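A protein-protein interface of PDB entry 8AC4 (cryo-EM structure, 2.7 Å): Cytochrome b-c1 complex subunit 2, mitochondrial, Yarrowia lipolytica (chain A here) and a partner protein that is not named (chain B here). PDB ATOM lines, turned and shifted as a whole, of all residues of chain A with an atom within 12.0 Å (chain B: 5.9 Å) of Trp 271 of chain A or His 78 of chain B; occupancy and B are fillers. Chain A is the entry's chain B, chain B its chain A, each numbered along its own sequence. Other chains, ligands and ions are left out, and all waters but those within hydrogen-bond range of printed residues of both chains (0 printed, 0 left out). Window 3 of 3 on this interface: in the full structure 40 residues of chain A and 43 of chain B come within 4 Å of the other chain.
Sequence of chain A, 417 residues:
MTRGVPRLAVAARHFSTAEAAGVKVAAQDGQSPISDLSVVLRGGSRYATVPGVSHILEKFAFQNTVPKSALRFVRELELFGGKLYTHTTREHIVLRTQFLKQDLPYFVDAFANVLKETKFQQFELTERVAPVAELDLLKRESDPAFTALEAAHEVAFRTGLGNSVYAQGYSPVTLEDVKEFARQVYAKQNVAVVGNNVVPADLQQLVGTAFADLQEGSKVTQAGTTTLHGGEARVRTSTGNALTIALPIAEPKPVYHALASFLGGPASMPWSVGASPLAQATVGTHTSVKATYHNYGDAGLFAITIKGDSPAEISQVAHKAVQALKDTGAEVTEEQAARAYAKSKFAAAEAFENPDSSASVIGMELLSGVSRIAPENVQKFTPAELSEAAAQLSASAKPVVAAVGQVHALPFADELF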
ATOM      1  N   GLY A 265     -14.481  -5.326   5.951  1.00  0.00           N
ATOM      2  CA  GLY A 265     -15.363  -4.182   6.098  1.00  0.00           C
ATOM      3  C   GLY A 265     -16.447  -4.398   7.155  1.00  0.00           C
ATOM      4  O   GLY A 265     -16.566  -3.574   8.064  1.00  0.00           O
ATOM      5  N   PRO A 266     -17.296  -5.456   7.051  1.00  0.00           N
ATOM      6  CA  PRO A 266     -18.299  -5.736   8.083  1.00  0.00           C
ATOM      7  C   PRO A 266     -17.645  -6.331   9.332  1.00  0.00           C
ATOM      8  O   PRO A 266     -16.546  -6.882   9.258  1.00  0.00           O
ATOM      9  CB  PRO A 266     -19.278  -6.700   7.391  1.00  0.00           C
ATOM     10  CG  PRO A 266     -18.429  -7.422   6.361  1.00  0.00           C
ATOM     11  CD  PRO A 266     -17.366  -6.428   5.943  1.00  0.00           C
ATOM     12  N   ALA A 267     -18.320  -6.172  10.482  1.00  0.00           N
ATOM     13  CA  ALA A 267     -17.782  -6.572  11.775  1.00  0.00           C
ATOM     14  C   ALA A 267     -18.101  -8.041  12.066  1.00  0.00           C
ATOM     15  O   ALA A 267     -19.116  -8.576  11.621  1.00  0.00           O
ATOM     16  CB  ALA A 267     -18.281  -5.640  12.858  1.00  0.00           C
ATOM     17  N   SER A 268     -17.212  -8.690  12.826  1.00  0.00           N
ATOM     18  CA  SER A 268     -17.332 -10.111  13.110  1.00  0.00           C
ATOM     19  C   SER A 268     -17.838 -10.335  14.533  1.00  0.00           C
ATOM     20  O   SER A 268     -17.620 -11.392  15.125  1.00  0.00           O
ATOM     21  CB  SER A 268     -16.017 -10.791  12.878  1.00  0.00           C
ATOM     22  OG  SER A 268     -15.747 -10.860  11.494  1.00  0.00           O
ATOM     23  N   MET A 269     -18.546  -9.333  15.065  1.00  0.00           N
ATOM     24  CA  MET A 269     -18.857  -9.204  16.479  1.00  0.00           C
ATOM     25  C   MET A 269     -19.875  -8.083  16.624  1.00  0.00           C
ATOM     26  O   MET A 269     -19.714  -7.046  15.992  1.00  0.00           O
ATOM     27  CB  MET A 269     -17.589  -8.728  17.177  1.00  0.00           C
ATOM     28  CG  MET A 269     -17.482  -9.085  18.611  1.00  0.00           C
ATOM     29  SD  MET A 269     -15.743  -9.137  19.084  1.00  0.00           S
ATOM     30  CE  MET A 269     -15.486  -7.472  19.696  1.00  0.00           C
ATOM     31  N   PRO A 270     -20.889  -8.184  17.509  1.00  0.00           N
ATOM     32  CA  PRO A 270     -21.857  -7.100  17.682  1.00  0.00           C
ATOM     33  C   PRO A 270     -21.209  -5.869  18.309  1.00  0.00           C
ATOM     34  O   PRO A 270     -20.263  -5.994  19.084  1.00  0.00           O
ATOM     35  CB  PRO A 270     -22.876  -7.690  18.664  1.00  0.00           C
ATOM     36  CG  PRO A 270     -22.640  -9.184  18.601  1.00  0.00           C
ATOM     37  CD  PRO A 270     -21.149  -9.328  18.390  1.00  0.00           C
ATOM     38  N   TRP A 271     -21.720  -4.683  17.950  1.00  0.00           N
ATOM     39  CA  TRP A 271     -21.319  -3.421  18.563  1.00  0.00           C
ATOM     40  C   TRP A 271     -19.816  -3.178  18.418  1.00  0.00           C
ATOM     41  O   TRP A 271     -19.210  -2.507  19.251  1.00  0.00           O
ATOM     42  CB  TRP A 271     -21.718  -3.372  20.045  1.00  0.00           C
ATOM     43  CG  TRP A 271     -22.996  -4.077  20.373  1.00  0.00           C
ATOM     44  CD1 TRP A 271     -23.151  -5.198  21.138  1.00  0.00           C
ATOM     45  CD2 TRP A 271     -24.313  -3.694  19.945  1.00  0.00           C
ATOM     46  NE1 TRP A 271     -24.476  -5.534  21.222  1.00  0.00           N
ATOM     47  CE2 TRP A 271     -25.212  -4.638  20.491  1.00  0.00           C
ATOM     48  CE3 TRP A 271     -24.815  -2.659  19.144  1.00  0.00           C
ATOM     49  CZ2 TRP A 271     -26.588  -4.567  20.269  1.00  0.00           C
ATOM     50  CZ3 TRP A 271     -26.174  -2.592  18.924  1.00  0.00           C
ATOM     51  CH2 TRP A 271     -27.046  -3.534  19.479  1.00  0.00           C
ATOM     52  N   SER A 272     -19.206  -3.749  17.382  1.00  0.00           N
ATOM     53  CA  SER A 272     -17.778  -3.561  17.186  1.00  0.00           C
ATOM     54  C   SER A 272     -17.538  -2.946  15.815  1.00  0.00           C
ATOM     55  O   SER A 272     -18.451  -2.869  14.995  1.00  0.00           O
ATOM     56  CB  SER A 272     -17.035  -4.855  17.376  1.00  0.00           C
ATOM     57  OG  SER A 272     -17.650  -5.608  18.410  1.00  0.00           O
ATOM     58  N   VAL A 273     -16.303  -2.488  15.591  1.00  0.00           N
ATOM     59  CA  VAL A 273     -15.930  -1.946  14.297  1.00  0.00           C
ATOM     60  C   VAL A 273     -15.326  -3.050  13.432  1.00  0.00           C
ATOM     61  O   VAL A 273     -15.729  -3.194  12.282  1.00  0.00           O
ATOM     62  CB  VAL A 273     -15.080  -0.661  14.406  1.00  0.00           C
ATOM     63  CG1 VAL A 273     -13.801  -0.686  13.580  1.00  0.00           C
ATOM     64  CG2 VAL A 273     -15.896   0.571  14.042  1.00  0.00           C
ATOM     65  N   GLY A 274     -14.398  -3.828  13.997  1.00  0.00           N
ATOM     66  CA  GLY A 274     -13.744  -4.893  13.255  1.00  0.00           C
ATOM     67  C   GLY A 274     -12.253  -4.617  13.119  1.00  0.00           C
ATOM     68  O   GLY A 274     -11.813  -3.488  13.316  1.00  0.00           O
ATOM     69  N   ALA A 275     -11.483  -5.662  12.806  1.00  0.00           N
ATOM     70  CA  ALA A 275     -10.032  -5.552  12.763  1.00  0.00           C
ATOM     71  C   ALA A 275      -9.537  -5.554  11.319  1.00  0.00           C
ATOM     72  O   ALA A 275      -8.328  -5.555  11.069  1.00  0.00           O
ATOM     73  CB  ALA A 275      -9.415  -6.656  13.588  1.00  0.00           C
ATOM     74  N   ALA A 279     -12.612  -1.819   7.828  1.00  0.00           N
ATOM     75  CA  ALA A 279     -13.473  -1.607   8.975  1.00  0.00           C
ATOM     76  C   ALA A 279     -12.883  -0.486   9.825  1.00  0.00           C
ATOM     77  O   ALA A 279     -13.620   0.351  10.341  1.00  0.00           O
ATOM     78  CB  ALA A 279     -13.606  -2.896   9.737  1.00  0.00           C
ATOM     79  N   GLN A 280     -11.543  -0.467   9.897  1.00  0.00           N
ATOM     80  CA  GLN A 280     -10.782   0.484  10.694  1.00  0.00           C
ATOM     81  C   GLN A 280     -10.790   1.859  10.027  1.00  0.00           C
ATOM     82  O   GLN A 280     -10.360   2.847  10.621  1.00  0.00           O
ATOM     83  CB  GLN A 280      -9.364  -0.043  10.934  1.00  0.00           C
ATOM     84  CG  GLN A 280      -9.262  -1.069  12.061  1.00  0.00           C
ATOM     85  CD  GLN A 280      -9.534  -0.513  13.440  1.00  0.00           C
ATOM     86  OE1 GLN A 280      -9.193   0.625  13.759  1.00  0.00           O
ATOM     87  NE2 GLN A 280     -10.136  -1.331  14.288  1.00  0.00           N
ATOM     88  N   THR A 282     -13.513   3.252   9.132  1.00  0.00           N
ATOM     89  CA  THR A 282     -14.812   3.839   9.416  1.00  0.00           C
ATOM     90  C   THR A 282     -14.842   4.439  10.820  1.00  0.00           C
ATOM     91  O   THR A 282     -15.913   4.828  11.280  1.00  0.00           O
ATOM     92  CB  THR A 282     -15.952   2.812   9.325  1.00  0.00           C
ATOM     93  OG1 THR A 282     -15.938   1.997  10.502  1.00  0.00           O
ATOM     94  CG2 THR A 282     -15.925   1.941   8.088  1.00  0.00           C
ATOM     95  N   VAL A 283     -13.698   4.455  11.523  1.00  0.00           N
ATOM     96  CA  VAL A 283     -13.732   4.795  12.940  1.00  0.00           C
ATOM     97  C   VAL A 283     -14.052   6.278  13.120  1.00  0.00           C
ATOM     98  O   VAL A 283     -13.408   7.146  12.529  1.00  0.00           O
ATOM     99  CB  VAL A 283     -12.498   4.324  13.738  1.00  0.00           C
ATOM    100  CG1 VAL A 283     -12.435   2.805  13.814  1.00  0.00           C
ATOM    101  CG2 VAL A 283     -11.187   4.909  13.228  1.00  0.00           C
ATOM    102  N   GLY A 284     -15.082   6.538  13.934  1.00  0.00           N
ATOM    103  CA  GLY A 284     -15.537   7.885  14.233  1.00  0.00           C
ATOM    104  C   GLY A 284     -16.651   8.337  13.292  1.00  0.00           C
ATOM    105  O   GLY A 284     -17.086   9.488  13.345  1.00  0.00           O
ATOM    106  N   THR A 285     -17.096   7.414  12.432  1.00  0.00           N
ATOM    107  CA  THR A 285     -18.147   7.686  11.468  1.00  0.00           C
ATOM    108  C   THR A 285     -19.223   6.608  11.579  1.00  0.00           C
ATOM    109  O   THR A 285     -18.929   5.455  11.887  1.00  0.00           O
ATOM    110  CB  THR A 285     -17.603   7.765  10.032  1.00  0.00           C
ATOM    111  OG1 THR A 285     -16.935   6.531   9.754  1.00  0.00           O
ATOM    112  CG2 THR A 285     -16.631   8.901   9.798  1.00  0.00           C
ATOM    113  N   HIS A 286     -20.471   7.013  11.323  1.00  0.00           N
ATOM    114  CA  HIS A 286     -21.579   6.085  11.179  1.00  0.00           C
ATOM    115  C   HIS A 286     -21.688   5.693   9.709  1.00  0.00           C
ATOM    116  O   HIS A 286     -22.648   6.042   9.024  1.00  0.00           O
ATOM    117  CB  HIS A 286     -22.868   6.671  11.780  1.00  0.00           C
ATOM    118  CG  HIS A 286     -22.674   7.277  13.130  1.00  0.00           C
ATOM    119  ND1 HIS A 286     -22.224   6.544  14.214  1.00  0.00           N
ATOM    120  CD2 HIS A 286     -22.853   8.540  13.574  1.00  0.00           C
ATOM    121  CE1 HIS A 286     -22.137   7.331  15.268  1.00  0.00           C
ATOM    122  NE2 HIS A 286     -22.520   8.561  14.902  1.00  0.00           N
ATOM    123  N   THR A 287     -20.648   5.011   9.233  1.00  0.00           N
ATOM    124  CA  THR A 287     -20.585   4.528   7.869  1.00  0.00           C
ATOM    125  C   THR A 287     -20.248   3.048   7.917  1.00  0.00           C
ATOM    126  O   THR A 287     -19.565   2.591   8.831  1.00  0.00           O
ATOM    127  CB  THR A 287     -19.512   5.255   7.050  1.00  0.00           C
ATOM    128  OG1 THR A 287     -18.283   5.143   7.769  1.00  0.00           O
ATOM    129  CG2 THR A 287     -19.842   6.702   6.750  1.00  0.00           C
ATOM    130  N   SER A 288     -20.757   2.315   6.933  1.00  0.00           N
ATOM    131  CA  SER A 288     -20.356   0.935   6.759  1.00  0.00           C
ATOM    132  C   SER A 288     -19.686   0.776   5.403  1.00  0.00           C
ATOM    133  O   SER A 288     -19.896   1.577   4.496  1.00  0.00           O
ATOM    134  CB  SER A 288     -21.507  -0.011   6.949  1.00  0.00           C
ATOM    135  OG  SER A 288     -22.663   0.478   6.296  1.00  0.00           O
ATOM    136  N   ALA B  73     -29.712  -6.010  31.015  1.00  0.00           N
ATOM    137  CA  ALA B  73     -29.432  -7.182  30.206  1.00  0.00           C
ATOM    138  C   ALA B  73     -28.942  -6.762  28.822  1.00  0.00           C
ATOM    139  O   ALA B  73     -28.048  -7.393  28.264  1.00  0.00           O
ATOM    140  CB  ALA B  73     -30.660  -8.049  30.126  1.00  0.00           C
ATOM    141  N   HIS B  74     -29.537  -5.702  28.273  1.00  0.00           N
ATOM    142  CA  HIS B  74     -29.134  -5.237  26.959  1.00  0.00           C
ATOM    143  C   HIS B  74     -27.780  -4.547  27.047  1.00  0.00           C
ATOM    144  O   HIS B  74     -26.978  -4.596  26.116  1.00  0.00           O
ATOM    145  CB  HIS B  74     -30.196  -4.317  26.368  1.00  0.00           C
ATOM    146  CG  HIS B  74     -29.843  -3.910  24.984  1.00  0.00           C
ATOM    147  ND1 HIS B  74     -29.163  -2.748  24.707  1.00  0.00           N
ATOM    148  CD2 HIS B  74     -30.082  -4.507  23.792  1.00  0.00           C
ATOM    149  CE1 HIS B  74     -28.981  -2.648  23.402  1.00  0.00           C
ATOM    150  NE2 HIS B  74     -29.530  -3.720  22.818  1.00  0.00           N
ATOM    151  N   PHE B  75     -27.566  -3.861  28.168  1.00  0.00           N
ATOM    152  CA  PHE B  75     -26.317  -3.168  28.402  1.00  0.00           C
ATOM    153  C   PHE B  75     -25.188  -4.184  28.410  1.00  0.00           C
ATOM    154  O   PHE B  75     -24.155  -3.953  27.796  1.00  0.00           O
ATOM    155  CB  PHE B  75     -26.329  -2.482  29.765  1.00  0.00           C
ATOM    156  CG  PHE B  75     -25.576  -1.184  29.779  1.00  0.00           C
ATOM    157  CD1 PHE B  75     -24.191  -1.158  29.703  1.00  0.00           C
ATOM    158  CD2 PHE B  75     -26.261   0.020  29.864  1.00  0.00           C
ATOM    159  CE1 PHE B  75     -23.505   0.048  29.689  1.00  0.00           C
ATOM    160  CE2 PHE B  75     -25.575   1.224  29.872  1.00  0.00           C
ATOM    161  CZ  PHE B  75     -24.201   1.233  29.786  1.00  0.00           C
ATOM    162  N   PHE B  76     -25.421  -5.308  29.093  1.00  0.00           N
ATOM    163  CA  PHE B  76     -24.398  -6.325  29.236  1.00  0.00           C
ATOM    164  C   PHE B  76     -23.975  -6.884  27.882  1.00  0.00           C
ATOM    165  O   PHE B  76     -22.792  -7.098  27.647  1.00  0.00           O
ATOM    166  CB  PHE B  76     -24.841  -7.444  30.176  1.00  0.00           C
ATOM    167  CG  PHE B  76     -23.789  -8.514  30.240  1.00  0.00           C
ATOM    168  CD1 PHE B  76     -22.628  -8.313  30.972  1.00  0.00           C
ATOM    169  CD2 PHE B  76     -23.911  -9.679  29.496  1.00  0.00           C
ATOM    170  CE1 PHE B  76     -21.639  -9.287  31.010  1.00  0.00           C
ATOM    171  CE2 PHE B  76     -22.924 -10.655  29.540  1.00  0.00           C
ATOM    172  CZ  PHE B  76     -21.784 -10.452  30.285  1.00  0.00           C
ATOM    173  N   GLU B  77     -24.949  -7.123  27.004  1.00  0.00           N
ATOM    174  CA  GLU B  77     -24.709  -7.570  25.640  1.00  0.00           C
ATOM    175  C   GLU B  77     -23.665  -6.701  24.936  1.00  0.00           C
ATOM    176  O   GLU B  77     -22.790  -7.257  24.275  1.00  0.00           O
ATOM    177  CB  GLU B  77     -26.041  -7.609  24.904  1.00  0.00           C
ATOM    178  CG  GLU B  77     -25.970  -8.193  23.512  1.00  0.00           C
ATOM    179  CD  GLU B  77     -27.172  -7.887  22.627  1.00  0.00           C
ATOM    180  OE1 GLU B  77     -28.288  -7.659  23.168  1.00  0.00           O
ATOM    181  OE2 GLU B  77     -27.001  -7.897  21.382  1.00  0.00           O
ATOM    182  N   HIS B  78     -23.696  -5.372  25.150  1.00  0.00           N
ATOM    183  CA  HIS B  78     -22.709  -4.463  24.562  1.00  0.00           C
ATOM    184  C   HIS B  78     -21.338  -4.669  25.206  1.00  0.00           C
ATOM    185  O   HIS B  78     -20.318  -4.789  24.523  1.00  0.00           O
ATOM    186  CB  HIS B  78     -23.116  -2.990  24.710  1.00  0.00           C
ATOM    187  CG  HIS B  78     -24.219  -2.540  23.815  1.00  0.00           C
ATOM    188  ND1 HIS B  78     -24.050  -1.546  22.873  1.00  0.00           N
ATOM    189  CD2 HIS B  78     -25.509  -2.928  23.709  1.00  0.00           C
ATOM    190  CE1 HIS B  78     -25.190  -1.335  22.235  1.00  0.00           C
ATOM    191  NE2 HIS B  78     -26.104  -2.174  22.724  1.00  0.00           N
ATOM    192  N   LEU B  79     -21.323  -4.866  26.527  1.00  0.00           N
ATOM    193  CA  LEU B  79     -20.069  -4.906  27.257  1.00  0.00           C
ATOM    194  C   LEU B  79     -19.392  -6.262  27.149  1.00  0.00           C
ATOM    195  O   LEU B  79     -18.214  -6.374  27.472  1.00  0.00           O
ATOM    196  CB  LEU B  79     -20.375  -4.618  28.718  1.00  0.00           C
ATOM    197  CG  LEU B  79     -20.026  -3.236  29.247  1.00  0.00           C
ATOM    198  CD1 LEU B  79     -19.613  -2.295  28.136  1.00  0.00           C
ATOM    199  CD2 LEU B  79     -21.224  -2.680  29.969  1.00  0.00           C
ATOM    200  N   ALA B  80     -20.160  -7.280  26.760  1.00  0.00           N
ATOM    201  CA  ALA B  80     -19.624  -8.622  26.664  1.00  0.00           C
ATOM    202  C   ALA B  80     -18.532  -8.657  25.597  1.00  0.00           C
ATOM    203  O   ALA B  80     -17.601  -9.456  25.677  1.00  0.00           O
ATOM    204  CB  ALA B  80     -20.736  -9.595  26.388  1.00  0.00           C
ATOM    205  N   PHE B  81     -18.623  -7.724  24.647  1.00  0.00           N
ATOM    206  CA  PHE B  81     -17.680  -7.701  23.544  1.00  0.00           C
ATOM    207  C   PHE B  81     -16.677  -6.563  23.708  1.00  0.00           C
ATOM    208  O   PHE B  81     -16.036  -6.124  22.751  1.00  0.00           O
ATOM    209  CB  PHE B  81     -18.457  -7.622  22.233  1.00  0.00           C
ATOM    210  CG  PHE B  81     -19.397  -8.780  22.038  1.00  0.00           C
ATOM    211  CD1 PHE B  81     -18.924 -10.035  21.679  1.00  0.00           C
ATOM    212  CD2 PHE B  81     -20.758  -8.624  22.253  1.00  0.00           C
ATOM    213  CE1 PHE B  81     -19.798 -11.094  21.488  1.00  0.00           C
ATOM    214  CE2 PHE B  81     -21.629  -9.691  22.085  1.00  0.00           C
ATOM    215  CZ  PHE B  81     -21.147 -10.927  21.712  1.00  0.00           C
ATOM    216  N   LYS B  82     -16.580  -6.034  24.925  1.00  0.00           N
ATOM    217  CA  LYS B  82     -15.739  -4.877  25.176  1.00  0.00           C
ATOM    218  C   LYS B  82     -14.474  -5.303  25.915  1.00  0.00           C
ATOM    219  O   LYS B  82     -13.761  -4.442  26.424  1.00  0.00           O
ATOM    220  CB  LYS B  82     -16.481  -3.799  25.981  1.00  0.00           C
ATOM    221  CG  LYS B  82     -17.256  -2.735  25.209  1.00  0.00           C
ATOM    222  CD  LYS B  82     -16.926  -2.635  23.755  1.00  0.00           C
ATOM    223  CE  LYS B  82     -18.167  -2.563  22.900  1.00  0.00           C
ATOM    224  NZ  LYS B  82     -18.319  -3.859  22.206  1.00  0.00           N
ATOM    225  N   GLN B  89     -10.231  -5.453  24.242  1.00  0.00           N
ATOM    226  CA  GLN B  89     -11.256  -5.291  23.218  1.00  0.00           C
ATOM    227  C   GLN B  89     -10.657  -5.637  21.855  1.00  0.00           C
ATOM    228  O   GLN B  89     -11.294  -6.284  21.023  1.00  0.00           O
ATOM    229  CB  GLN B  89     -11.805  -3.859  23.243  1.00  0.00           C
ATOM    230  CG  GLN B  89     -13.228  -3.685  22.712  1.00  0.00           C
ATOM    231  CD  GLN B  89     -13.335  -3.392  21.232  1.00  0.00           C
ATOM    232  OE1 GLN B  89     -12.403  -2.884  20.609  1.00  0.00           O
ATOM    233  NE2 GLN B  89     -14.484  -3.705  20.651  1.00  0.00           N
ATOM    234  N   ALA B 105     -25.082 -11.907  19.258  1.00  0.00           N
ATOM    235  CA  ALA B 105     -25.827 -11.966  20.502  1.00  0.00           C
ATOM    236  C   ALA B 105     -27.160 -11.253  20.319  1.00  0.00           C
ATOM    237  O   ALA B 105     -27.246 -10.328  19.518  1.00  0.00           O
ATOM    238  CB  ALA B 105     -25.024 -11.316  21.594  1.00  0.00           C
ATOM    239  N   GLU B 147     -20.228   3.184  26.392  1.00  0.00           N
ATOM    240  CA  GLU B 147     -21.375   2.521  25.777  1.00  0.00           C
ATOM    241  C   GLU B 147     -22.657   3.254  26.138  1.00  0.00           C
ATOM    242  O   GLU B 147     -23.663   3.151  25.439  1.00  0.00           O
ATOM    243  CB  GLU B 147     -21.553   1.082  26.263  1.00  0.00           C
ATOM    244  CG  GLU B 147     -20.704   0.068  25.513  1.00  0.00           C
ATOM    245  CD  GLU B 147     -20.533   0.191  24.007  1.00  0.00           C
ATOM    246  OE1 GLU B 147     -21.413  -0.292  23.261  1.00  0.00           O
ATOM    247  OE2 GLU B 147     -19.506   0.757  23.583  1.00  0.00           O
ATOM    248  N   VAL B 150     -23.608   5.262  23.287  1.00  0.00           N
ATOM    249  CA  VAL B 150     -23.962   4.428  22.149  1.00  0.00           C
ATOM    250  C   VAL B 150     -25.400   3.951  22.303  1.00  0.00           C
ATOM    251  O   VAL B 150     -26.171   3.957  21.346  1.00  0.00           O
ATOM    252  CB  VAL B 150     -23.008   3.224  22.038  1.00  0.00           C
ATOM    253  CG1 VAL B 150     -23.379   2.289  20.895  1.00  0.00           C
ATOM    254  CG2 VAL B 150     -21.563   3.672  21.916  1.00  0.00           C
ATOM    255  N   ILE B 151     -25.722   3.518  23.524  1.00  0.00           N
ATOM    256  CA  ILE B 151     -27.025   2.976  23.850  1.00  0.00           C
ATOM    257  C   ILE B 151     -28.030   4.119  23.890  1.00  0.00           C
ATOM    258  O   ILE B 151     -29.184   3.932  23.507  1.00  0.00           O
ATOM    259  CB  ILE B 151     -26.957   2.167  25.160  1.00  0.00           C
ATOM    260  CG1 ILE B 151     -26.231   0.837  24.935  1.00  0.00           C
ATOM    261  CG2 ILE B 151     -28.343   1.952  25.746  1.00  0.00           C
ATOM    262  CD1 ILE B 151     -25.759   0.158  26.198  1.00  0.00           C
ATOM    263  N   GLU B 154     -29.217   4.733  20.572  1.00  0.00           N
ATOM    264  CA  GLU B 154     -30.029   3.646  20.040  1.00  0.00           C
ATOM    265  C   GLU B 154     -31.500   3.905  20.346  1.00  0.00           C
ATOM    266  O   GLU B 154     -32.362   3.451  19.601  1.00  0.00           O
ATOM    267  CB  GLU B 154     -29.670   2.306  20.679  1.00  0.00           C
ATOM    268  CG  GLU B 154     -28.636   1.476  19.947  1.00  0.00           C
ATOM    269  CD  GLU B 154     -28.372   0.154  20.651  1.00  0.00           C
ATOM    270  OE1 GLU B 154     -28.063   0.167  21.867  1.00  0.00           O
ATOM    271  OE2 GLU B 154     -28.514  -0.890  19.995  1.00  0.00           O
ATOM    272  N   LEU B 185     -34.445  -2.035  25.951  1.00  0.00           N
ATOM    273  CA  LEU B 185     -33.440  -0.993  26.063  1.00  0.00           C
ATOM    274  C   LEU B 185     -33.489  -0.320  27.429  1.00  0.00           C
ATOM    275  O   LEU B 185     -32.454   0.083  27.946  1.00  0.00           O
ATOM    276  CB  LEU B 185     -33.645   0.033  24.949  1.00  0.00           C
ATOM    277  CG  LEU B 185     -32.630  -0.027  23.817  1.00  0.00           C
ATOM    278  CD1 LEU B 185     -32.815   1.158  22.872  1.00  0.00           C
ATOM    279  CD2 LEU B 185     -31.214  -0.013  24.360  1.00  0.00           C
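CE of Met 269 of chain A touches O of Phe 81 of chain B, at 3.4 Å. Pro 270 of chain A touches Phe 81 of chain B. Pro 270 of chain A touches Ala 105 of chain B. Trp 271 of chain A touches His 74 of chain B. Trp 271 of chain A touches His 78 of chain B. Trp 271 of chain A touches Glu 154 of chain B.
OE2 of Glu 77 of chain B is in hydrogen-bond range of NE1 of Trp 271 of chain A, 3.5 Å away. NZ of Lys 82 of chain B is in hydrogen-bond range of O of Trp 271 of chain A, at 3.4 Å.
Hydrophobic or aromatic side chains of chain A within 4 Å of the printed part of chain B: Met 269, Pro 270 and Trp 271. Of the 17 printed residues of chain B, 7 touch a printed residue of chain A. Printed residues of chain B that touch a printed residue of chain A: His 74, Glu 77, His 78, Phe 81, Lys 82, Ala 105 and Glu 154. Along chain B the printed residues that touch a printed residue of chain A span positions 74 to 154. Among the printed residues, no Asp or Glu carboxylate lies within 4 Å of a Lys or Arg side-chain nitrogen of the other chain.
The side-chain amino group (NZ) of Lys 82 of chain B sits at hydrogen-bond distance from the backbone carbonyl oxygen (O) of His 78 of chain B. ND1 of His 78 of chain B lies within hydrogen-bond range of OE1 of Glu 147 of chain B (2.9 Å). The side-chain carboxylate (OE1) of Glu 154 of chain B lies within hydrogen-bond range of a ring nitrogen (NE2) of His 78 of chain B, at 3.2 Å. The backbone carbonyl oxygen of Met 269 of chain A lies close to the side-chain hydroxyl of Ser 272 of chain A. O of Pro 270 of chain A lies within hydrogen-bond range of OG of Ser 272 of chain A, 2.7 Å away.
Of the printed residues of chain B, Met 269 of chain A touches Phe 81. Printed residues of chain B within 4 Å of Pro 270 of chain A: Phe 81 (3.7 Å) and Ala 105 (3.7 Å). Of the printed residues of chain B, Trp 271 of chain A touches His 74, Glu 77, His 78, Lys 82 and Glu 154. Of the printed residues of chain A, His 74 of chain B touches Trp 271. No residue of chain A comes within 4 Å of Phe 75 of chain B. No residue of chain A comes within 4 Å of Phe 76 of chain B. Glu 77 of chain B touches just one residue of chain A: Trp 271. His 78 of chain B touches one residue of chain A. Leu 79 of chain B touches none of the printed residues of chain A. Phe 81 of chain B touches two residues of chain A. No residue of chain A comes within 4 Å of Val 150 of chain B. Printed residues of chain A within 4 Å of Glu 154 of chain B: Trp 271. The nearest printed residue of chain A that does not touch His 74 of chain B is Pro 270 of chain A (8.8 Å).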
